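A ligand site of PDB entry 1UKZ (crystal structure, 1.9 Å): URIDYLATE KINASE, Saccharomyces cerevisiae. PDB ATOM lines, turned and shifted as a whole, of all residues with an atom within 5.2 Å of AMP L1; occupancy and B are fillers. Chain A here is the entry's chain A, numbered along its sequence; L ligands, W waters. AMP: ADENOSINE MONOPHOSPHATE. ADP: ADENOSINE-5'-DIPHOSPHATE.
The backbone NH of Gln 73 sits at hydrogen-bond distance from the backbone carbonyl oxygen of Cys 68, 2.7 Å away. The backbone NH (N) of Arg 106 is in hydrogen-bond range of the side-chain amide oxygen (OE1) of Gln 110 (2.7 Å). The side-chain carboxylate (OD2) of Asp 149 lies within salt-bridge range of the guanidinium group (NH2) of Arg 147, 2.8 Å away. The guanidinium group (NE) of Arg 51 sits close to the backbone carbonyl oxygen (O) of Gly 47, 3.5 Å away. The side-chain hydroxyl (OG1) of Thr 80 sits at hydrogen-bond distance from the backbone carbonyl oxygen (O) of Val 75, at 3.3 Å. OD2 of Asp 149 lies within salt-bridge range of NE of Arg 158 (3.6 Å). N of Ala 46 is in hydrogen-bond range of O of Asp 102, at 3.0 Å. The backbone NH (N) of Gly 47 sits close to the side-chain hydroxyl (OG) of Ser 45 (3.5 Å).
Water W3 lies within hydrogen-bond range of an oxygen (O3') of AMP L1, the backbone carbonyl oxygen of Ile 69 and the side-chain carboxylate of Asp 149. Water W7 lies within hydrogen-bond range of an oxygen (O1P) of AMP L1 (2.6 Å), an oxygen (O3B) of ADP L2 (2.7 Å), the guanidinium group (NH2) of Arg 141 (3.0 Å) and the guanidinium group (NH2) of Arg 158 (3.0 Å). Water W2 lies within hydrogen-bond range of O2P of AMP L1 (2.6 Å), NH2 of Arg 51 (2.9 Å) and OG of Ser 45 (3.2 Å). Water W4 lies within hydrogen-bond range of O3P of AMP L1 (2.7 Å), OG of Ser 45 (2.9 Å), N of Gly 47 (3.0 Å) and O of Asp 102 (3.3 Å). Water W6 lies within hydrogen-bond range of O3P of AMP L1, NH2 of Arg 106 and O3B of ADP L2. Water W1 bridges O of Gly 72 and O3' of AMP L1.
Residues that only touch AMP L1: Leu 50, Ile 69, Ile 74, Thr 80, Cys 68, Phe 104, Ala 46, Gly 47 and Asp 149. Hydrophobic or aromatic side chains that line AMP L1: Ala 46, Leu 50, Ile 69, Ile 74, Val 75 and Phe 104. Of the 24 residues printed, 17 come within 4 Å of AMP L1. Along chain A the residues within 4 Å of AMP L1 span positions 46 to 158. The nearest printed residue that does not touch AMP L1 is Gly 72 (4.02 Å).
The backbone carbonyl oxygen (O) of Gln 73 is in hydrogen-bond range of an oxygen (O2') of AMP L1, 2.7 Å away. The guanidinium group (NH1) of Arg 106 is in salt-bridge range of an oxygen (O3P) of AMP L1. The backbone carbonyl oxygen (O) of Gly 103 lies within hydrogen-bond range of a nitrogen (N6) of AMP L1. An oxygen (O1P) of AMP L1 is in salt-bridge range of the guanidinium group (NH2) of Arg 147 (2.9 Å). NH1 of Arg 51 is in salt-bridge range of O2P of AMP L1 (2.9 Å). The backbone NH (N) of Val 75 lies within hydrogen-bond range of a nitrogen (N3) of AMP L1 (3.0 Å). NE2 of Gln 110 is in hydrogen-bond range of N1 of AMP L1 (3.0 Å). The guanidinium group of Arg 158 lies within salt-bridge range of an oxygen (O1P) of AMP L1 (3.6 Å). The guanidinium group of Arg 141 lies within salt-bridge range of an oxygen (O1A) of ADP L2 (2.9 Å).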
ATOM      1  N   PRO A  24      19.792  27.084 -16.431  1.00  0.00           N
ATOM      2  CA  PRO A  24      19.068  26.814 -15.186  1.00  0.00           C
ATOM      3  C   PRO A  24      18.447  28.111 -14.638  1.00  0.00           C
ATOM      4  O   PRO A  24      19.109  29.149 -14.618  1.00  0.00           O
ATOM      5  CB  PRO A  24      20.153  26.249 -14.274  1.00  0.00           C
ATOM      6  CG  PRO A  24      21.403  26.944 -14.739  1.00  0.00           C
ATOM      7  CD  PRO A  24      21.254  26.924 -16.258  1.00  0.00           C
ATOM      8  N   SER A  45      10.356  16.539 -17.547  1.00  0.00           N
ATOM      9  CA  SER A  45      11.540  17.277 -17.140  1.00  0.00           C
ATOM     10  C   SER A  45      12.703  16.291 -16.990  1.00  0.00           C
ATOM     11  O   SER A  45      12.614  15.341 -16.220  1.00  0.00           O
ATOM     12  CB  SER A  45      11.286  18.012 -15.818  1.00  0.00           C
ATOM     13  OG  SER A  45      12.484  18.508 -15.250  1.00  0.00           O
ATOM     14  N   ALA A  46      13.801  16.541 -17.691  1.00  0.00           N
ATOM     15  CA  ALA A  46      14.930  15.640 -17.605  1.00  0.00           C
ATOM     16  C   ALA A  46      15.487  15.692 -16.183  1.00  0.00           C
ATOM     17  O   ALA A  46      15.796  14.648 -15.615  1.00  0.00           O
ATOM     18  CB  ALA A  46      15.980  16.010 -18.630  1.00  0.00           C
ATOM     19  N   GLY A  47      15.550  16.865 -15.584  1.00  0.00           N
ATOM     20  CA  GLY A  47      16.051  16.973 -14.228  1.00  0.00           C
ATOM     21  C   GLY A  47      15.206  16.166 -13.257  1.00  0.00           C
ATOM     22  O   GLY A  47      15.716  15.492 -12.358  1.00  0.00           O
ATOM     23  N   ASP A  48      13.895  16.244 -13.416  1.00  0.00           N
ATOM     24  CA  ASP A  48      12.981  15.502 -12.576  1.00  0.00           C
ATOM     25  C   ASP A  48      13.163  13.995 -12.747  1.00  0.00           C
ATOM     26  O   ASP A  48      13.165  13.249 -11.768  1.00  0.00           O
ATOM     27  CB  ASP A  48      11.512  15.830 -12.914  1.00  0.00           C
ATOM     28  CG  ASP A  48      11.035  17.125 -12.307  1.00  0.00           C
ATOM     29  OD1 ASP A  48      11.790  17.743 -11.526  1.00  0.00           O
ATOM     30  OD2 ASP A  48       9.893  17.525 -12.617  1.00  0.00           O
ATOM     31  N   LEU A  50      15.750  12.412 -13.679  1.00  0.00           N
ATOM     32  CA  LEU A  50      17.029  12.047 -13.099  1.00  0.00           C
ATOM     33  C   LEU A  50      16.948  12.021 -11.592  1.00  0.00           C
ATOM     34  O   LEU A  50      17.438  11.098 -10.956  1.00  0.00           O
ATOM     35  CB  LEU A  50      18.107  13.026 -13.535  1.00  0.00           C
ATOM     36  CG  LEU A  50      18.542  12.848 -14.981  1.00  0.00           C
ATOM     37  CD1 LEU A  50      19.431  14.025 -15.344  1.00  0.00           C
ATOM     38  CD2 LEU A  50      19.259  11.508 -15.161  1.00  0.00           C
ATOM     39  N   ARG A  51      16.333  13.045 -11.014  1.00  0.00           N
ATOM     40  CA  ARG A  51      16.194  13.086  -9.574  1.00  0.00           C
ATOM     41  C   ARG A  51      15.358  11.920  -9.037  1.00  0.00           C
ATOM     42  O   ARG A  51      15.615  11.415  -7.943  1.00  0.00           O
ATOM     43  CB  ARG A  51      15.626  14.409  -9.139  1.00  0.00           C
ATOM     44  CG  ARG A  51      16.647  15.512  -9.145  1.00  0.00           C
ATOM     45  CD  ARG A  51      16.055  16.789  -8.589  1.00  0.00           C
ATOM     46  NE  ARG A  51      15.107  17.403  -9.519  1.00  0.00           N
ATOM     47  CZ  ARG A  51      15.449  18.176 -10.535  1.00  0.00           C
ATOM     48  NH1 ARG A  51      16.732  18.443 -10.761  1.00  0.00           N
ATOM     49  NH2 ARG A  51      14.527  18.653 -11.359  1.00  0.00           N
ATOM     50  N   CYS A  68      26.747  13.914 -10.397  1.00  0.00           N
ATOM     51  CA  CYS A  68      26.641  14.719 -11.604  1.00  0.00           C
ATOM     52  C   CYS A  68      25.862  15.998 -11.299  1.00  0.00           C
ATOM     53  O   CYS A  68      26.314  17.088 -11.650  1.00  0.00           O
ATOM     54  CB  CYS A  68      25.954  13.930 -12.707  1.00  0.00           C
ATOM     55  SG  CYS A  68      27.034  12.768 -13.522  1.00  0.00           S
ATOM     56  N   ILE A  69      24.717  15.878 -10.626  1.00  0.00           N
ATOM     57  CA  ILE A  69      23.875  17.022 -10.274  1.00  0.00           C
ATOM     58  C   ILE A  69      24.614  18.055  -9.412  1.00  0.00           C
ATOM     59  O   ILE A  69      24.592  19.253  -9.720  1.00  0.00           O
ATOM     60  CB  ILE A  69      22.533  16.571  -9.587  1.00  0.00           C
ATOM     61  CG1 ILE A  69      21.629  15.884 -10.617  1.00  0.00           C
ATOM     62  CG2 ILE A  69      21.823  17.766  -8.916  1.00  0.00           C
ATOM     63  CD1 ILE A  69      20.316  15.330 -10.050  1.00  0.00           C
ATOM     64  N   GLY A  72      27.011  19.845 -11.441  1.00  0.00           N
ATOM     65  CA  GLY A  72      26.423  20.475 -12.608  1.00  0.00           C
ATOM     66  C   GLY A  72      26.853  19.801 -13.889  1.00  0.00           C
ATOM     67  O   GLY A  72      26.902  20.427 -14.941  1.00  0.00           O
ATOM     68  N   GLN A  73      27.156  18.515 -13.806  1.00  0.00           N
ATOM     69  CA  GLN A  73      27.607  17.737 -14.963  1.00  0.00           C
ATOM     70  C   GLN A  73      26.464  17.096 -15.716  1.00  0.00           C
ATOM     71  O   GLN A  73      25.418  16.795 -15.134  1.00  0.00           O
ATOM     72  CB  GLN A  73      28.539  16.607 -14.523  1.00  0.00           C
ATOM     73  CG  GLN A  73      29.784  17.049 -13.778  1.00  0.00           C
ATOM     74  CD  GLN A  73      30.662  15.866 -13.345  1.00  0.00           C
ATOM     75  OE1 GLN A  73      31.866  16.028 -13.182  1.00  0.00           O
ATOM     76  NE2 GLN A  73      30.065  14.688 -13.159  1.00  0.00           N
ATOM     77  N   ILE A  74      26.693  16.843 -16.992  1.00  0.00           N
ATOM     78  CA  ILE A  74      25.708  16.173 -17.834  1.00  0.00           C
ATOM     79  C   ILE A  74      25.811  14.654 -17.571  1.00  0.00           C
ATOM     80  O   ILE A  74      26.858  14.050 -17.766  1.00  0.00           O
ATOM     81  CB  ILE A  74      25.960  16.486 -19.358  1.00  0.00           C
ATOM     82  CG1 ILE A  74      25.767  17.982 -19.617  1.00  0.00           C
ATOM     83  CG2 ILE A  74      25.029  15.677 -20.262  1.00  0.00           C
ATOM     84  CD1 ILE A  74      24.415  18.529 -19.161  1.00  0.00           C
ATOM     85  N   VAL A  75      24.733  14.075 -17.049  1.00  0.00           N
ATOM     86  CA  VAL A  75      24.670  12.645 -16.783  1.00  0.00           C
ATOM     87  C   VAL A  75      24.775  11.937 -18.125  1.00  0.00           C
ATOM     88  O   VAL A  75      24.185  12.387 -19.107  1.00  0.00           O
ATOM     89  CB  VAL A  75      23.337  12.275 -16.080  1.00  0.00           C
ATOM     90  CG1 VAL A  75      23.174  10.759 -15.930  1.00  0.00           C
ATOM     91  CG2 VAL A  75      23.263  12.944 -14.709  1.00  0.00           C
ATOM     92  N   THR A  80      20.313   8.861 -19.222  1.00  0.00           N
ATOM     93  CA  THR A  80      19.337   9.899 -19.501  1.00  0.00           C
ATOM     94  C   THR A  80      18.334   9.504 -20.569  1.00  0.00           C
ATOM     95  O   THR A  80      17.123   9.678 -20.388  1.00  0.00           O
ATOM     96  CB  THR A  80      20.038  11.191 -19.929  1.00  0.00           C
ATOM     97  OG1 THR A  80      21.020  11.535 -18.943  1.00  0.00           O
ATOM     98  CG2 THR A  80      19.036  12.337 -20.058  1.00  0.00           C
ATOM     99  N   ASP A 102      11.521  19.275 -21.226  1.00  0.00           N
ATOM    100  CA  ASP A 102      12.264  20.366 -20.653  1.00  0.00           C
ATOM    101  C   ASP A 102      13.632  19.931 -20.112  1.00  0.00           C
ATOM    102  O   ASP A 102      13.754  18.959 -19.381  1.00  0.00           O
ATOM    103  CB  ASP A 102      11.290  21.085 -19.676  1.00  0.00           C
ATOM    104  CG  ASP A 102      11.898  21.478 -18.337  1.00  0.00           C
ATOM    105  OD1 ASP A 102      13.075  21.815 -18.232  1.00  0.00           O
ATOM    106  OD2 ASP A 102      11.106  21.521 -17.361  1.00  0.00           O
ATOM    107  N   GLY A 103      14.664  20.645 -20.550  1.00  0.00           N
ATOM    108  CA  GLY A 103      16.011  20.352 -20.094  1.00  0.00           C
ATOM    109  C   GLY A 103      16.743  19.273 -20.850  1.00  0.00           C
ATOM    110  O   GLY A 103      17.730  18.729 -20.377  1.00  0.00           O
ATOM    111  N   PHE A 104      16.268  18.949 -22.045  1.00  0.00           N
ATOM    112  CA  PHE A 104      16.894  17.940 -22.857  1.00  0.00           C
ATOM    113  C   PHE A 104      16.626  18.342 -24.283  1.00  0.00           C
ATOM    114  O   PHE A 104      15.517  18.766 -24.589  1.00  0.00           O
ATOM    115  CB  PHE A 104      16.278  16.575 -22.570  1.00  0.00           C
ATOM    116  CG  PHE A 104      16.820  15.474 -23.433  1.00  0.00           C
ATOM    117  CD1 PHE A 104      16.436  15.360 -24.767  1.00  0.00           C
ATOM    118  CD2 PHE A 104      17.723  14.548 -22.920  1.00  0.00           C
ATOM    119  CE1 PHE A 104      16.959  14.366 -25.579  1.00  0.00           C
ATOM    120  CE2 PHE A 104      18.234  13.551 -23.725  1.00  0.00           C
ATOM    121  CZ  PHE A 104      17.861  13.464 -25.048  1.00  0.00           C
ATOM    122  N   PRO A 105      17.612  18.220 -25.185  1.00  0.00           N
ATOM    123  CA  PRO A 105      18.985  17.719 -24.976  1.00  0.00           C
ATOM    124  C   PRO A 105      19.943  18.780 -24.502  1.00  0.00           C
ATOM    125  O   PRO A 105      19.930  19.915 -24.977  1.00  0.00           O
ATOM    126  CB  PRO A 105      19.374  17.220 -26.358  1.00  0.00           C
ATOM    127  CG  PRO A 105      18.722  18.197 -27.254  1.00  0.00           C
ATOM    128  CD  PRO A 105      17.361  18.420 -26.626  1.00  0.00           C
ATOM    129  N   ARG A 106      20.835  18.400 -23.598  1.00  0.00           N
ATOM    130  CA  ARG A 106      21.786  19.339 -23.056  1.00  0.00           C
ATOM    131  C   ARG A 106      23.202  19.104 -23.530  1.00  0.00           C
ATOM    132  O   ARG A 106      24.124  19.787 -23.119  1.00  0.00           O
ATOM    133  CB  ARG A 106      21.732  19.316 -21.523  1.00  0.00           C
ATOM    134  CG  ARG A 106      20.659  20.218 -20.975  1.00  0.00           C
ATOM    135  CD  ARG A 106      20.548  20.137 -19.480  1.00  0.00           C
ATOM    136  NE  ARG A 106      19.904  21.337 -18.950  1.00  0.00           N
ATOM    137  CZ  ARG A 106      18.955  21.357 -18.024  1.00  0.00           C
ATOM    138  NH1 ARG A 106      18.501  20.225 -17.507  1.00  0.00           N
ATOM    139  NH2 ARG A 106      18.484  22.513 -17.579  1.00  0.00           N
ATOM    140  N   GLN A 110      23.440  13.324 -26.849  1.00  0.00           N
ATOM    141  CA  GLN A 110      22.063  12.958 -26.542  1.00  0.00           C
ATOM    142  C   GLN A 110      21.077  13.596 -27.502  1.00  0.00           C
ATOM    143  O   GLN A 110      19.989  13.060 -27.730  1.00  0.00           O
ATOM    144  CB  GLN A 110      21.718  13.259 -25.078  1.00  0.00           C
ATOM    145  CG  GLN A 110      22.042  14.652 -24.606  1.00  0.00           C
ATOM    146  CD  GLN A 110      21.579  14.912 -23.192  1.00  0.00           C
ATOM    147  OE1 GLN A 110      20.683  15.727 -22.972  1.00  0.00           O
ATOM    148  NE2 GLN A 110      22.179  14.227 -22.223  1.00  0.00           N
ATOM    149  N   ARG A 141      15.230  30.590  -5.566  1.00  0.00           N
ATOM    150  CA  ARG A 141      14.694  29.235  -5.581  1.00  0.00           C
ATOM    151  C   ARG A 141      15.389  28.368  -4.551  1.00  0.00           C
ATOM    152  O   ARG A 141      14.764  27.533  -3.914  1.00  0.00           O
ATOM    153  CB  ARG A 141      14.832  28.599  -6.962  1.00  0.00           C
ATOM    154  CG  ARG A 141      13.941  27.388  -7.148  1.00  0.00           C
ATOM    155  CD  ARG A 141      13.981  26.873  -8.556  1.00  0.00           C
ATOM    156  NE  ARG A 141      15.216  26.149  -8.809  1.00  0.00           N
ATOM    157  CZ  ARG A 141      15.585  25.670  -9.992  1.00  0.00           C
ATOM    158  NH1 ARG A 141      14.806  25.833 -11.053  1.00  0.00           N
ATOM    159  NH2 ARG A 141      16.740  25.033 -10.102  1.00  0.00           N
ATOM    160  N   ARG A 147      16.531  22.962  -3.135  1.00  0.00           N
ATOM    161  CA  ARG A 147      17.061  21.927  -4.025  1.00  0.00           C
ATOM    162  C   ARG A 147      18.542  21.888  -3.733  1.00  0.00           C
ATOM    163  O   ARG A 147      19.187  22.931  -3.625  1.00  0.00           O
ATOM    164  CB  ARG A 147      16.865  22.329  -5.488  1.00  0.00           C
ATOM    165  CG  ARG A 147      16.200  21.285  -6.315  1.00  0.00           C
ATOM    166  CD  ARG A 147      15.917  21.816  -7.702  1.00  0.00           C
ATOM    167  NE  ARG A 147      17.102  21.852  -8.545  1.00  0.00           N
ATOM    168  CZ  ARG A 147      17.058  21.898  -9.874  1.00  0.00           C
ATOM    169  NH1 ARG A 147      15.888  21.923 -10.492  1.00  0.00           N
ATOM    170  NH2 ARG A 147      18.181  21.951 -10.587  1.00  0.00           N
ATOM    171  N   ASP A 149      21.311  21.331  -5.525  1.00  0.00           N
ATOM    172  CA  ASP A 149      22.171  22.053  -6.446  1.00  0.00           C
ATOM    173  C   ASP A 149      21.914  23.552  -6.595  1.00  0.00           C
ATOM    174  O   ASP A 149      22.580  24.232  -7.368  1.00  0.00           O
ATOM    175  CB  ASP A 149      22.180  21.381  -7.819  1.00  0.00           C
ATOM    176  CG  ASP A 149      20.790  21.318  -8.474  1.00  0.00           C
ATOM    177  OD1 ASP A 149      19.776  21.371  -7.757  1.00  0.00           O
ATOM    178  OD2 ASP A 149      20.718  21.196  -9.695  1.00  0.00           O
ATOM    179  N   ARG A 158      26.833  24.801 -13.120  1.00  0.00           N
ATOM    180  CA  ARG A 158      25.691  24.634 -14.026  1.00  0.00           C
ATOM    181  C   ARG A 158      25.723  25.685 -15.151  1.00  0.00           C
ATOM    182  O   ARG A 158      25.486  25.349 -16.308  1.00  0.00           O
ATOM    183  CB  ARG A 158      24.375  24.703 -13.236  1.00  0.00           C
ATOM    184  CG  ARG A 158      24.221  23.516 -12.299  1.00  0.00           C
ATOM    185  CD  ARG A 158      23.308  23.848 -11.162  1.00  0.00           C
ATOM    186  NE  ARG A 158      21.940  24.003 -11.623  1.00  0.00           N
ATOM    187  CZ  ARG A 158      20.955  24.461 -10.865  1.00  0.00           C
ATOM    188  NH1 ARG A 158      21.197  24.824  -9.606  1.00  0.00           N
ATOM    189  NH2 ARG A 158      19.717  24.450 -11.320  1.00  0.00           N
HETATM  190  P   AMP L   1      17.558  20.738 -13.906  1.00  0.00           P
HETATM  191  O1P AMP L   1      18.266  22.010 -13.485  1.00  0.00           O
HETATM  192  O2P AMP L   1      16.626  20.387 -12.911  1.00  0.00           O
HETATM  193  O3P AMP L   1      17.045  20.836 -15.228  1.00  0.00           O
HETATM  194  O5' AMP L   1      18.737  19.680 -13.933  1.00  0.00           O
HETATM  195  C5' AMP L   1      19.462  19.329 -12.758  1.00  0.00           C
HETATM  196  C4' AMP L   1      20.742  18.586 -13.031  1.00  0.00           C
HETATM  197  O4' AMP L   1      20.449  17.273 -13.553  1.00  0.00           O
HETATM  198  C3' AMP L   1      21.582  19.274 -14.147  1.00  0.00           C
HETATM  199  O3' AMP L   1      22.412  20.329 -13.677  1.00  0.00           O
HETATM  200  C2' AMP L   1      22.466  18.115 -14.644  1.00  0.00           C
HETATM  201  O2' AMP L   1      23.389  17.773 -13.624  1.00  0.00           O
HETATM  202  C1' AMP L   1      21.199  17.229 -14.731  1.00  0.00           C
HETATM  203  N9  AMP L   1      20.603  16.960 -15.983  1.00  0.00           N
HETATM  204  C8  AMP L   1      19.484  17.660 -16.299  1.00  0.00           C
HETATM  205  N7  AMP L   1      19.169  17.467 -17.532  1.00  0.00           N
HETATM  206  C5  AMP L   1      20.084  16.612 -18.093  1.00  0.00           C
HETATM  207  C6  AMP L   1      20.225  16.089 -19.368  1.00  0.00           C
HETATM  208  N6  AMP L   1      19.408  16.452 -20.358  1.00  0.00           N
HETATM  209  N1  AMP L   1      21.253  15.231 -19.560  1.00  0.00           N
HETATM  210  C2  AMP L   1      22.080  14.947 -18.563  1.00  0.00           C
HETATM  211  N3  AMP L   1      22.081  15.393 -17.296  1.00  0.00           N
HETATM  212  C4  AMP L   1      21.027  16.255 -17.089  1.00  0.00           C
HETATM  213  PB  ADP L   2      14.156  26.335 -14.909  1.00  0.00           P
HETATM  214  O1B ADP L   2      13.261  25.207 -14.948  1.00  0.00           O
HETATM  215  O2B ADP L   2      14.538  26.872 -16.177  1.00  0.00           O
HETATM  216  O3B ADP L   2      15.405  25.894 -14.166  1.00  0.00           O
HETATM  217  PA  ADP L   2      12.206  27.683 -13.122  1.00  0.00           P
HETATM  218  O1A ADP L   2      12.277  26.856 -11.981  1.00  0.00           O
HETATM  219  O2A ADP L   2      10.981  27.595 -13.855  1.00  0.00           O
HETATM  220  O3A ADP L   2      13.446  27.387 -14.024  1.00  0.00           O
HETATM  221  O5' ADP L   2      12.363  29.142 -12.657  1.00  0.00           O
HETATM  222  C5' ADP L   2      13.462  29.460 -11.789  1.00  0.00           C
HETATM  223  C4' ADP L   2      13.008  30.136 -10.503  1.00  0.00           C
HETATM  224  O4' ADP L   2      12.579  31.474 -10.798  1.00  0.00           O
HETATM  225  C3' ADP L   2      11.808  29.467  -9.754  1.00  0.00           C
HETATM  226  O3' ADP L   2      11.861  29.826  -8.399  1.00  0.00           O
HETATM  227  C2' ADP L   2      10.587  30.087 -10.441  1.00  0.00           C
HETATM  228  O2' ADP L   2       9.465  30.316  -9.563  1.00  0.00           O
HETATM  229  C1' ADP L   2      11.174  31.379 -11.025  1.00  0.00           C
HETATM  230  N9  ADP L   2      10.566  32.115 -12.070  1.00  0.00           N
HETATM  231  C8  ADP L   2      10.248  31.490 -13.224  1.00  0.00           C
HETATM  232  N7  ADP L   2       9.968  32.334 -14.141  1.00  0.00           N
HETATM  233  C5  ADP L   2      10.068  33.586 -13.622  1.00  0.00           C
HETATM  234  C6  ADP L   2       9.848  34.875 -14.138  1.00  0.00           C
HETATM  235  N6  ADP L   2       9.506  35.089 -15.393  1.00  0.00           N
HETATM  236  N1  ADP L   2      10.019  35.887 -13.283  1.00  0.00           N
HETATM  237  C2  ADP L   2      10.381  35.672 -12.014  1.00  0.00           C
HETATM  238  N3  ADP L   2      10.622  34.511 -11.410  1.00  0.00           N
HETATM  239  C4  ADP L   2      10.434  33.460 -12.266  1.00  0.00           C
HETATM  240  O   HOH W   1      24.286  21.167 -15.654  1.00  0.00           O
HETATM  241  O   HOH W   2      14.075  20.624 -13.466  1.00  0.00           O
HETATM  242  O   HOH W   3      22.813  20.466 -11.147  1.00  0.00           O
HETATM  243  O   HOH W   4      14.917  19.656 -16.423  1.00  0.00           O
HETATM  244  O   HOH W   5      20.686  22.718 -13.998  1.00  0.00           O
HETATM  245  O   HOH W   6      16.623  23.550 -15.714  1.00  0.00           O
HETATM  246  O   HOH W   7      17.219  24.338 -12.975  1.00  0.00           O
